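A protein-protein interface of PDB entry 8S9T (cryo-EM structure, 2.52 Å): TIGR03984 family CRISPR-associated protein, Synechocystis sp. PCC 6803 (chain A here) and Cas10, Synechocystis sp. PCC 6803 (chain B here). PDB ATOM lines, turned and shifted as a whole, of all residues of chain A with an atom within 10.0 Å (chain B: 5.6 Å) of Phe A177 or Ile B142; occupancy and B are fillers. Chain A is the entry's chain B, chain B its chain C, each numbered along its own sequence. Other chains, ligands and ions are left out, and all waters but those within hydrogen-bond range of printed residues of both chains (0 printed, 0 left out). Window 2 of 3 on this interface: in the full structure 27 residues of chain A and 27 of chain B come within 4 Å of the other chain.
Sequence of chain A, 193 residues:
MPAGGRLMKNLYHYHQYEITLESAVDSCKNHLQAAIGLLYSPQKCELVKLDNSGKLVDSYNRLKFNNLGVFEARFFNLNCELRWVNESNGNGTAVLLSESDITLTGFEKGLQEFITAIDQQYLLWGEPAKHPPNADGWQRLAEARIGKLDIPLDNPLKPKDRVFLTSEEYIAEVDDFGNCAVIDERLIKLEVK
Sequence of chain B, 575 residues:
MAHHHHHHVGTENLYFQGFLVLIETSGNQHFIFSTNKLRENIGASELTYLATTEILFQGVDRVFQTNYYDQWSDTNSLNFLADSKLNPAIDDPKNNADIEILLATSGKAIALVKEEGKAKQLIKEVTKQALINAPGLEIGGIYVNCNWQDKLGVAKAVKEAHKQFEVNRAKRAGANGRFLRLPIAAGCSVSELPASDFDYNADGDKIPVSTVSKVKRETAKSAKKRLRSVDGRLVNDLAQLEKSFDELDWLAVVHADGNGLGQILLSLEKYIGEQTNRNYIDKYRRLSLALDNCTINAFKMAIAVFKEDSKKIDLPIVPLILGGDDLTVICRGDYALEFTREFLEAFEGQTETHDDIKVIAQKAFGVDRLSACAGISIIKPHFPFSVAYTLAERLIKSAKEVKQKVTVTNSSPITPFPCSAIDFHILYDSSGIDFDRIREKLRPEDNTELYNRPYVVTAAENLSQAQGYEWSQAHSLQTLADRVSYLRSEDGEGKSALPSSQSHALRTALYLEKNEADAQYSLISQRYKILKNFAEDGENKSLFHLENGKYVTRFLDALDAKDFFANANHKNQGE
N of Val A174 is in hydrogen-bond range of O of Asn A179, at 2.7 Å. OD2 of Asp A175 lies within hydrogen-bond range of ND2 of Asn A179. O of Leu B22 is in hydrogen-bond range of N of Ile B142 (2.9 Å).
Among the printed residues, merely in contact across the chains: Ile A115 with Lys B124 (3.8 Å), Glu A173 with Lys B124 (3.0 Å), Asp A176 with Lys B120 (3.2 Å), Phe A177 with Lys B120 (3.5 Å), Phe A177 with Ile B123 (3.2 Å), Phe A177 with Gly B141 (3.8 Å), Phe A177 with Ile B142 (3.4 Å), Phe A177 with Tyr B143 (3.6 Å), Phe A177 with Asn B168 (3.0 Å), Gly A178 with Lys B120 (3.7 Å), Gly A178 with Ile B123 (3.9 Å), Asn A179 with Ile B123 (3.4 Å) and Asn A179 with Gly B140 (3.4 Å).
Of the printed residues of chain B, Glu A173 touches Lys B120 and Lys B124. Of the printed residues of chain B, Asp A176 touches Lys B120 (3.2 Å) and Tyr B143 (3.5 Å). Phe A177 touches six residues of chain B. No residue of chain A comes within 4 Å of Val B21. Of chain A, only Glu A173 (3.0 Å), Asp A176 (3.2 Å), Phe A177 (3.5 Å) and Gly A178 (3.7 Å) come within 4 Å of Lys B120. Gly B141 touches two residues of chain A. Of chain A, only Phe A177 comes within 4 Å of Ile B142. Of the printed residues of chain A, Tyr B143 touches Asp A176 (3.5 Å) and Phe A177 (3.6 Å). Ala B161 touches none of the printed residues of chain A. Printed residues of chain A within 4 Å of Asn B168: Phe A177 (3.0 Å). The nearest residue of chain A that does not touch Ile B142 is Asn A179 (5.3 Å).
OE1 of Glu A173 is in salt-bridge range of NZ of Lys B120 (3.0 Å). The side-chain hydroxyl (OH) of Tyr B143 sits at hydrogen-bond distance from the backbone carbonyl oxygen (O) of Asp A176. The backbone carbonyl oxygen (O) of Gly A178 lies close to the backbone NH (N) of Lys B124, 3.4 Å away. N of Gly B141 is in hydrogen-bond range of OD1 of Asn A179, at 2.8 Å. O of Lys B124 lies close to SG of Cys A180.
Hydrophobic or aromatic side chains of chain A that line the printed part of chain B: Ile A115 and Phe A177. Of the 18 printed residues of chain B, 8 touch a printed residue of chain A. Hydrophobic or aromatic side chains of chain B that line the printed part of chain A: Ile B123, Ile B142 and Tyr B143. Among the printed residues, Asp or Glu carboxylates within 4 Å of a Lys or Arg side-chain nitrogen of the other chain: Glu A173 with Lys B120 (3.0 Å).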
ATOM      1  N   ILE A 115       0.217 -39.752  19.183  1.00  0.00           N
ATOM      2  CA  ILE A 115      -0.871 -39.229  18.364  1.00  0.00           C
ATOM      3  C   ILE A 115      -1.846 -40.336  18.002  1.00  0.00           C
ATOM      4  O   ILE A 115      -3.065 -40.165  18.089  1.00  0.00           O
ATOM      5  CB  ILE A 115      -0.296 -38.559  17.106  1.00  0.00           C
ATOM      6  CG1 ILE A 115       0.670 -37.448  17.501  1.00  0.00           C
ATOM      7  CG2 ILE A 115      -1.406 -38.009  16.247  1.00  0.00           C
ATOM      8  CD1 ILE A 115       1.698 -37.160  16.449  1.00  0.00           C
ATOM      9  N   ALA A 172       4.171 -40.591  17.485  1.00  0.00           N
ATOM     10  CA  ALA A 172       4.269 -39.354  18.241  1.00  0.00           C
ATOM     11  C   ALA A 172       5.130 -38.363  17.474  1.00  0.00           C
ATOM     12  O   ALA A 172       5.848 -38.727  16.542  1.00  0.00           O
ATOM     13  CB  ALA A 172       4.865 -39.599  19.629  1.00  0.00           C
ATOM     14  N   GLU A 173       5.017 -37.092  17.854  1.00  0.00           N
ATOM     15  CA  GLU A 173       5.909 -36.058  17.342  1.00  0.00           C
ATOM     16  C   GLU A 173       7.305 -36.214  17.932  1.00  0.00           C
ATOM     17  O   GLU A 173       7.478 -36.156  19.154  1.00  0.00           O
ATOM     18  CB  GLU A 173       5.350 -34.682  17.662  1.00  0.00           C
ATOM     19  CG  GLU A 173       4.071 -34.363  16.934  1.00  0.00           C
ATOM     20  CD  GLU A 173       3.632 -32.945  17.168  1.00  0.00           C
ATOM     21  OE1 GLU A 173       2.971 -32.374  16.283  1.00  0.00           O
ATOM     22  OE2 GLU A 173       3.960 -32.395  18.239  1.00  0.00           O
ATOM     23  N   VAL A 174       8.299 -36.391  17.068  1.00  0.00           N
ATOM     24  CA  VAL A 174       9.689 -36.374  17.505  1.00  0.00           C
ATOM     25  C   VAL A 174      10.292 -34.969  17.519  1.00  0.00           C
ATOM     26  O   VAL A 174      11.146 -34.673  18.360  1.00  0.00           O
ATOM     27  CB  VAL A 174      10.510 -37.327  16.628  1.00  0.00           C
ATOM     28  CG1 VAL A 174      11.984 -37.271  16.995  1.00  0.00           C
ATOM     29  CG2 VAL A 174       9.996 -38.724  16.804  1.00  0.00           C
ATOM     30  N   ASP A 175       9.835 -34.079  16.645  1.00  0.00           N
ATOM     31  CA  ASP A 175      10.440 -32.770  16.475  1.00  0.00           C
ATOM     32  C   ASP A 175       9.456 -31.671  16.836  1.00  0.00           C
ATOM     33  O   ASP A 175       8.238 -31.848  16.756  1.00  0.00           O
ATOM     34  CB  ASP A 175      10.898 -32.532  15.034  1.00  0.00           C
ATOM     35  CG  ASP A 175      12.029 -33.427  14.623  1.00  0.00           C
ATOM     36  OD1 ASP A 175      12.721 -33.966  15.509  1.00  0.00           O
ATOM     37  OD2 ASP A 175      12.240 -33.571  13.404  1.00  0.00           O
ATOM     38  N   ASP A 176      10.010 -30.537  17.264  1.00  0.00           N
ATOM     39  CA  ASP A 176       9.234 -29.311  17.371  1.00  0.00           C
ATOM     40  C   ASP A 176       8.745 -28.806  16.022  1.00  0.00           C
ATOM     41  O   ASP A 176       7.824 -27.986  15.983  1.00  0.00           O
ATOM     42  CB  ASP A 176      10.070 -28.235  18.056  1.00  0.00           C
ATOM     43  CG  ASP A 176      10.532 -28.653  19.434  1.00  0.00           C
ATOM     44  OD1 ASP A 176       9.863 -29.505  20.051  1.00  0.00           O
ATOM     45  OD2 ASP A 176      11.567 -28.135  19.902  1.00  0.00           O
ATOM     46  N   PHE A 177       9.334 -29.266  14.918  1.00  0.00           N
ATOM     47  CA  PHE A 177       8.772 -28.994  13.600  1.00  0.00           C
ATOM     48  C   PHE A 177       7.513 -29.788  13.300  1.00  0.00           C
ATOM     49  O   PHE A 177       6.856 -29.504  12.298  1.00  0.00           O
ATOM     50  CB  PHE A 177       9.814 -29.234  12.507  1.00  0.00           C
ATOM     51  CG  PHE A 177      10.994 -28.329  12.611  1.00  0.00           C
ATOM     52  CD1 PHE A 177      10.825 -26.960  12.548  1.00  0.00           C
ATOM     53  CD2 PHE A 177      12.271 -28.834  12.752  1.00  0.00           C
ATOM     54  CE1 PHE A 177      11.894 -26.115  12.657  1.00  0.00           C
ATOM     55  CE2 PHE A 177      13.348 -27.986  12.853  1.00  0.00           C
ATOM     56  CZ  PHE A 177      13.160 -26.628  12.803  1.00  0.00           C
ATOM     57  N   GLY A 178       7.154 -30.757  14.134  1.00  0.00           N
ATOM     58  CA  GLY A 178       5.997 -31.591  13.891  1.00  0.00           C
ATOM     59  C   GLY A 178       6.263 -32.920  13.214  1.00  0.00           C
ATOM     60  O   GLY A 178       5.307 -33.643  12.937  1.00  0.00           O
ATOM     61  N   ASN A 179       7.513 -33.267  12.936  1.00  0.00           N
ATOM     62  CA  ASN A 179       7.816 -34.569  12.352  1.00  0.00           C
ATOM     63  C   ASN A 179       7.387 -35.697  13.284  1.00  0.00           C
ATOM     64  O   ASN A 179       7.804 -35.752  14.442  1.00  0.00           O
ATOM     65  CB  ASN A 179       9.306 -34.671  12.047  1.00  0.00           C
ATOM     66  CG  ASN A 179       9.748 -33.695  10.996  1.00  0.00           C
ATOM     67  OD1 ASN A 179       9.241 -33.702   9.883  1.00  0.00           O
ATOM     68  ND2 ASN A 179      10.671 -32.822  11.353  1.00  0.00           N
ATOM     69  N   CYS A 180       6.544 -36.588  12.772  1.00  0.00           N
ATOM     70  CA  CYS A 180       6.115 -37.785  13.479  1.00  0.00           C
ATOM     71  C   CYS A 180       7.086 -38.943  13.281  1.00  0.00           C
ATOM     72  O   CYS A 180       7.733 -39.069  12.241  1.00  0.00           O
ATOM     73  CB  CYS A 180       4.733 -38.204  12.994  1.00  0.00           C
ATOM     74  SG  CYS A 180       3.474 -37.019  13.333  1.00  0.00           S
ATOM     75  N   LEU B  20       7.918 -20.396   5.573  1.00  0.00           N
ATOM     76  CA  LEU B  20       8.122 -21.307   4.465  1.00  0.00           C
ATOM     77  C   LEU B  20       8.289 -22.714   5.016  1.00  0.00           C
ATOM     78  O   LEU B  20       9.186 -22.962   5.824  1.00  0.00           O
ATOM     79  CB  LEU B  20       9.336 -20.882   3.649  1.00  0.00           C
ATOM     80  CG  LEU B  20       9.619 -21.670   2.382  1.00  0.00           C
ATOM     81  CD1 LEU B  20       9.908 -20.691   1.292  1.00  0.00           C
ATOM     82  CD2 LEU B  20      10.795 -22.579   2.592  1.00  0.00           C
ATOM     83  N   VAL B  21       7.442 -23.632   4.561  1.00  0.00           N
ATOM     84  CA  VAL B  21       7.550 -25.047   4.898  1.00  0.00           C
ATOM     85  C   VAL B  21       8.227 -25.775   3.751  1.00  0.00           C
ATOM     86  O   VAL B  21       7.817 -25.644   2.596  1.00  0.00           O
ATOM     87  CB  VAL B  21       6.174 -25.658   5.200  1.00  0.00           C
ATOM     88  CG1 VAL B  21       6.276 -27.152   5.273  1.00  0.00           C
ATOM     89  CG2 VAL B  21       5.648 -25.120   6.501  1.00  0.00           C
ATOM     90  N   LEU B  22       9.279 -26.515   4.062  1.00  0.00           N
ATOM     91  CA  LEU B  22       9.891 -27.456   3.141  1.00  0.00           C
ATOM     92  C   LEU B  22       9.635 -28.860   3.663  1.00  0.00           C
ATOM     93  O   LEU B  22      10.043 -29.192   4.777  1.00  0.00           O
ATOM     94  CB  LEU B  22      11.387 -27.180   3.012  1.00  0.00           C
ATOM     95  CG  LEU B  22      12.332 -28.236   2.456  1.00  0.00           C
ATOM     96  CD1 LEU B  22      12.038 -28.504   1.009  1.00  0.00           C
ATOM     97  CD2 LEU B  22      13.746 -27.768   2.613  1.00  0.00           C
ATOM     98  N   ILE B  23       8.978 -29.681   2.855  1.00  0.00           N
ATOM     99  CA  ILE B  23       8.758 -31.088   3.153  1.00  0.00           C
ATOM    100  C   ILE B  23       9.489 -31.887   2.092  1.00  0.00           C
ATOM    101  O   ILE B  23       9.322 -31.633   0.896  1.00  0.00           O
ATOM    102  CB  ILE B  23       7.260 -31.436   3.176  1.00  0.00           C
ATOM    103  CG1 ILE B  23       6.596 -30.814   4.396  1.00  0.00           C
ATOM    104  CG2 ILE B  23       7.076 -32.919   3.229  1.00  0.00           C
ATOM    105  CD1 ILE B  23       5.107 -30.691   4.277  1.00  0.00           C
ATOM    106  N   ALA B 119       1.857 -24.310  10.050  1.00  0.00           N
ATOM    107  CA  ALA B 119       3.105 -24.834   9.514  1.00  0.00           C
ATOM    108  C   ALA B 119       3.462 -26.163  10.162  1.00  0.00           C
ATOM    109  O   ALA B 119       3.702 -27.160   9.473  1.00  0.00           O
ATOM    110  CB  ALA B 119       4.231 -23.824   9.724  1.00  0.00           C
ATOM    111  N   LYS B 120       3.498 -26.186  11.497  1.00  0.00           N
ATOM    112  CA  LYS B 120       3.764 -27.415  12.238  1.00  0.00           C
ATOM    113  C   LYS B 120       2.696 -28.471  11.984  1.00  0.00           C
ATOM    114  O   LYS B 120       3.010 -29.651  11.806  1.00  0.00           O
ATOM    115  CB  LYS B 120       3.866 -27.110  13.727  1.00  0.00           C
ATOM    116  CG  LYS B 120       4.506 -28.209  14.517  1.00  0.00           C
ATOM    117  CD  LYS B 120       4.579 -27.868  15.980  1.00  0.00           C
ATOM    118  CE  LYS B 120       3.231 -28.098  16.617  1.00  0.00           C
ATOM    119  NZ  LYS B 120       3.082 -29.517  17.043  1.00  0.00           N
ATOM    120  N   ILE B 123       3.162 -30.257   8.761  1.00  0.00           N
ATOM    121  CA  ILE B 123       4.260 -31.213   8.792  1.00  0.00           C
ATOM    122  C   ILE B 123       3.857 -32.474   9.545  1.00  0.00           C
ATOM    123  O   ILE B 123       4.141 -33.590   9.100  1.00  0.00           O
ATOM    124  CB  ILE B 123       5.508 -30.558   9.403  1.00  0.00           C
ATOM    125  CG1 ILE B 123       5.987 -29.409   8.522  1.00  0.00           C
ATOM    126  CG2 ILE B 123       6.618 -31.567   9.551  1.00  0.00           C
ATOM    127  CD1 ILE B 123       6.844 -28.416   9.241  1.00  0.00           C
ATOM    128  N   LYS B 124       3.175 -32.323  10.682  1.00  0.00           N
ATOM    129  CA  LYS B 124       2.652 -33.487  11.389  1.00  0.00           C
ATOM    130  C   LYS B 124       1.700 -34.293  10.521  1.00  0.00           C
ATOM    131  O   LYS B 124       1.783 -35.523  10.465  1.00  0.00           O
ATOM    132  CB  LYS B 124       1.939 -33.061  12.670  1.00  0.00           C
ATOM    133  CG  LYS B 124       1.715 -34.210  13.620  1.00  0.00           C
ATOM    134  CD  LYS B 124       0.791 -33.870  14.775  1.00  0.00           C
ATOM    135  CE  LYS B 124      -0.671 -33.949  14.370  1.00  0.00           C
ATOM    136  NZ  LYS B 124      -1.557 -33.612  15.519  1.00  0.00           N
ATOM    137  N   GLY B 140      10.533 -35.899   5.960  1.00  0.00           N
ATOM    138  CA  GLY B 140      10.593 -34.914   7.014  1.00  0.00           C
ATOM    139  C   GLY B 140      10.161 -33.560   6.494  1.00  0.00           C
ATOM    140  O   GLY B 140       9.969 -33.369   5.300  1.00  0.00           O
ATOM    141  N   GLY B 141      10.006 -32.624   7.419  1.00  0.00           N
ATOM    142  CA  GLY B 141       9.723 -31.256   7.048  1.00  0.00           C
ATOM    143  C   GLY B 141      10.322 -30.280   8.033  1.00  0.00           C
ATOM    144  O   GLY B 141      10.728 -30.639   9.139  1.00  0.00           O
ATOM    145  N   ILE B 142      10.382 -29.025   7.603  1.00  0.00           N
ATOM    146  CA  ILE B 142      10.911 -27.950   8.424  1.00  0.00           C
ATOM    147  C   ILE B 142      10.172 -26.677   8.050  1.00  0.00           C
ATOM    148  O   ILE B 142       9.668 -26.543   6.936  1.00  0.00           O
ATOM    149  CB  ILE B 142      12.440 -27.837   8.248  1.00  0.00           C
ATOM    150  CG1 ILE B 142      13.049 -27.029   9.384  1.00  0.00           C
ATOM    151  CG2 ILE B 142      12.785 -27.258   6.889  1.00  0.00           C
ATOM    152  CD1 ILE B 142      14.533 -27.105   9.434  1.00  0.00           C
ATOM    153  N   TYR B 143      10.075 -25.749   8.990  1.00  0.00           N
ATOM    154  CA  TYR B 143       9.569 -24.419   8.693  1.00  0.00           C
ATOM    155  C   TYR B 143      10.569 -23.367   9.145  1.00  0.00           C
ATOM    156  O   TYR B 143      11.223 -23.518  10.179  1.00  0.00           O
ATOM    157  CB  TYR B 143       8.195 -24.174   9.328  1.00  0.00           C
ATOM    158  CG  TYR B 143       8.117 -24.316  10.832  1.00  0.00           C
ATOM    159  CD1 TYR B 143       8.555 -23.305  11.667  1.00  0.00           C
ATOM    160  CD2 TYR B 143       7.591 -25.453  11.413  1.00  0.00           C
ATOM    161  CE1 TYR B 143       8.466 -23.418  13.027  1.00  0.00           C
ATOM    162  CE2 TYR B 143       7.510 -25.580  12.772  1.00  0.00           C
ATOM    163  CZ  TYR B 143       7.947 -24.556  13.578  1.00  0.00           C
ATOM    164  OH  TYR B 143       7.882 -24.667  14.949  1.00  0.00           O
ATOM    165  N   VAL B 144      10.687 -22.308   8.352  1.00  0.00           N
ATOM    166  CA  VAL B 144      11.501 -21.151   8.689  1.00  0.00           C
ATOM    167  C   VAL B 144      10.663 -19.900   8.494  1.00  0.00           C
ATOM    168  O   VAL B 144       9.688 -19.893   7.739  1.00  0.00           O
ATOM    169  CB  VAL B 144      12.791 -21.069   7.852  1.00  0.00           C
ATOM    170  CG1 VAL B 144      13.635 -22.295   8.067  1.00  0.00           C
ATOM    171  CG2 VAL B 144      12.448 -20.917   6.403  1.00  0.00           C
ATOM    172  N   ALA B 161      15.712 -22.744   4.929  1.00  0.00           N
ATOM    173  CA  ALA B 161      14.967 -23.991   5.065  1.00  0.00           C
ATOM    174  C   ALA B 161      15.761 -25.183   4.556  1.00  0.00           C
ATOM    175  O   ALA B 161      15.815 -26.229   5.209  1.00  0.00           O
ATOM    176  CB  ALA B 161      13.637 -23.880   4.328  1.00  0.00           C
ATOM    177  N   HIS B 162      16.364 -25.056   3.378  1.00  0.00           N
ATOM    178  CA  HIS B 162      17.166 -26.147   2.841  1.00  0.00           C
ATOM    179  C   HIS B 162      18.351 -26.485   3.735  1.00  0.00           C
ATOM    180  O   HIS B 162      18.531 -27.641   4.126  1.00  0.00           O
ATOM    181  CB  HIS B 162      17.626 -25.807   1.429  1.00  0.00           C
ATOM    182  CG  HIS B 162      16.556 -25.976   0.398  1.00  0.00           C
ATOM    183  ND1 HIS B 162      15.515 -25.088   0.255  1.00  0.00           N
ATOM    184  CD2 HIS B 162      16.359 -26.940  -0.529  1.00  0.00           C
ATOM    185  CE1 HIS B 162      14.724 -25.494  -0.720  1.00  0.00           C
ATOM    186  NE2 HIS B 162      15.215 -26.614  -1.215  1.00  0.00           N
ATOM    187  N   GLN B 164      18.924 -25.767   6.837  1.00  0.00           N
ATOM    188  CA  GLN B 164      18.505 -26.273   8.139  1.00  0.00           C
ATOM    189  C   GLN B 164      17.958 -27.689   8.055  1.00  0.00           C
ATOM    190  O   GLN B 164      18.055 -28.446   9.026  1.00  0.00           O
ATOM    191  CB  GLN B 164      17.462 -25.349   8.759  1.00  0.00           C
ATOM    192  CG  GLN B 164      17.998 -24.024   9.224  1.00  0.00           C
ATOM    193  CD  GLN B 164      19.050 -24.189  10.294  1.00  0.00           C
ATOM    194  OE1 GLN B 164      20.245 -24.236  10.009  1.00  0.00           O
ATOM    195  NE2 GLN B 164      18.607 -24.298  11.541  1.00  0.00           N
ATOM    196  N   PHE B 165      17.372 -28.055   6.919  1.00  0.00           N
ATOM    197  CA  PHE B 165      16.912 -29.423   6.715  1.00  0.00           C
ATOM    198  C   PHE B 165      18.065 -30.416   6.785  1.00  0.00           C
ATOM    199  O   PHE B 165      17.964 -31.451   7.451  1.00  0.00           O
ATOM    200  CB  PHE B 165      16.186 -29.497   5.370  1.00  0.00           C
ATOM    201  CG  PHE B 165      15.378 -30.737   5.163  1.00  0.00           C
ATOM    202  CD1 PHE B 165      15.984 -31.934   4.836  1.00  0.00           C
ATOM    203  CD2 PHE B 165      14.004 -30.706   5.283  1.00  0.00           C
ATOM    204  CE1 PHE B 165      15.239 -33.065   4.640  1.00  0.00           C
ATOM    205  CE2 PHE B 165      13.259 -31.842   5.085  1.00  0.00           C
ATOM    206  CZ  PHE B 165      13.878 -33.018   4.765  1.00  0.00           C
ATOM    207  N   ASN B 168      19.165 -31.060  10.352  1.00  0.00           N
ATOM    208  CA  ASN B 168      18.294 -32.011  11.037  1.00  0.00           C
ATOM    209  C   ASN B 168      18.537 -33.444  10.581  1.00  0.00           C
ATOM    210  O   ASN B 168      18.534 -34.365  11.404  1.00  0.00           O
ATOM    211  CB  ASN B 168      16.838 -31.620  10.846  1.00  0.00           C
ATOM    212  CG  ASN B 168      16.477 -30.390  11.622  1.00  0.00           C
ATOM    213  OD1 ASN B 168      17.311 -29.812  12.314  1.00  0.00           O
ATOM    214  ND2 ASN B 168      15.228 -29.973  11.512  1.00  0.00           N
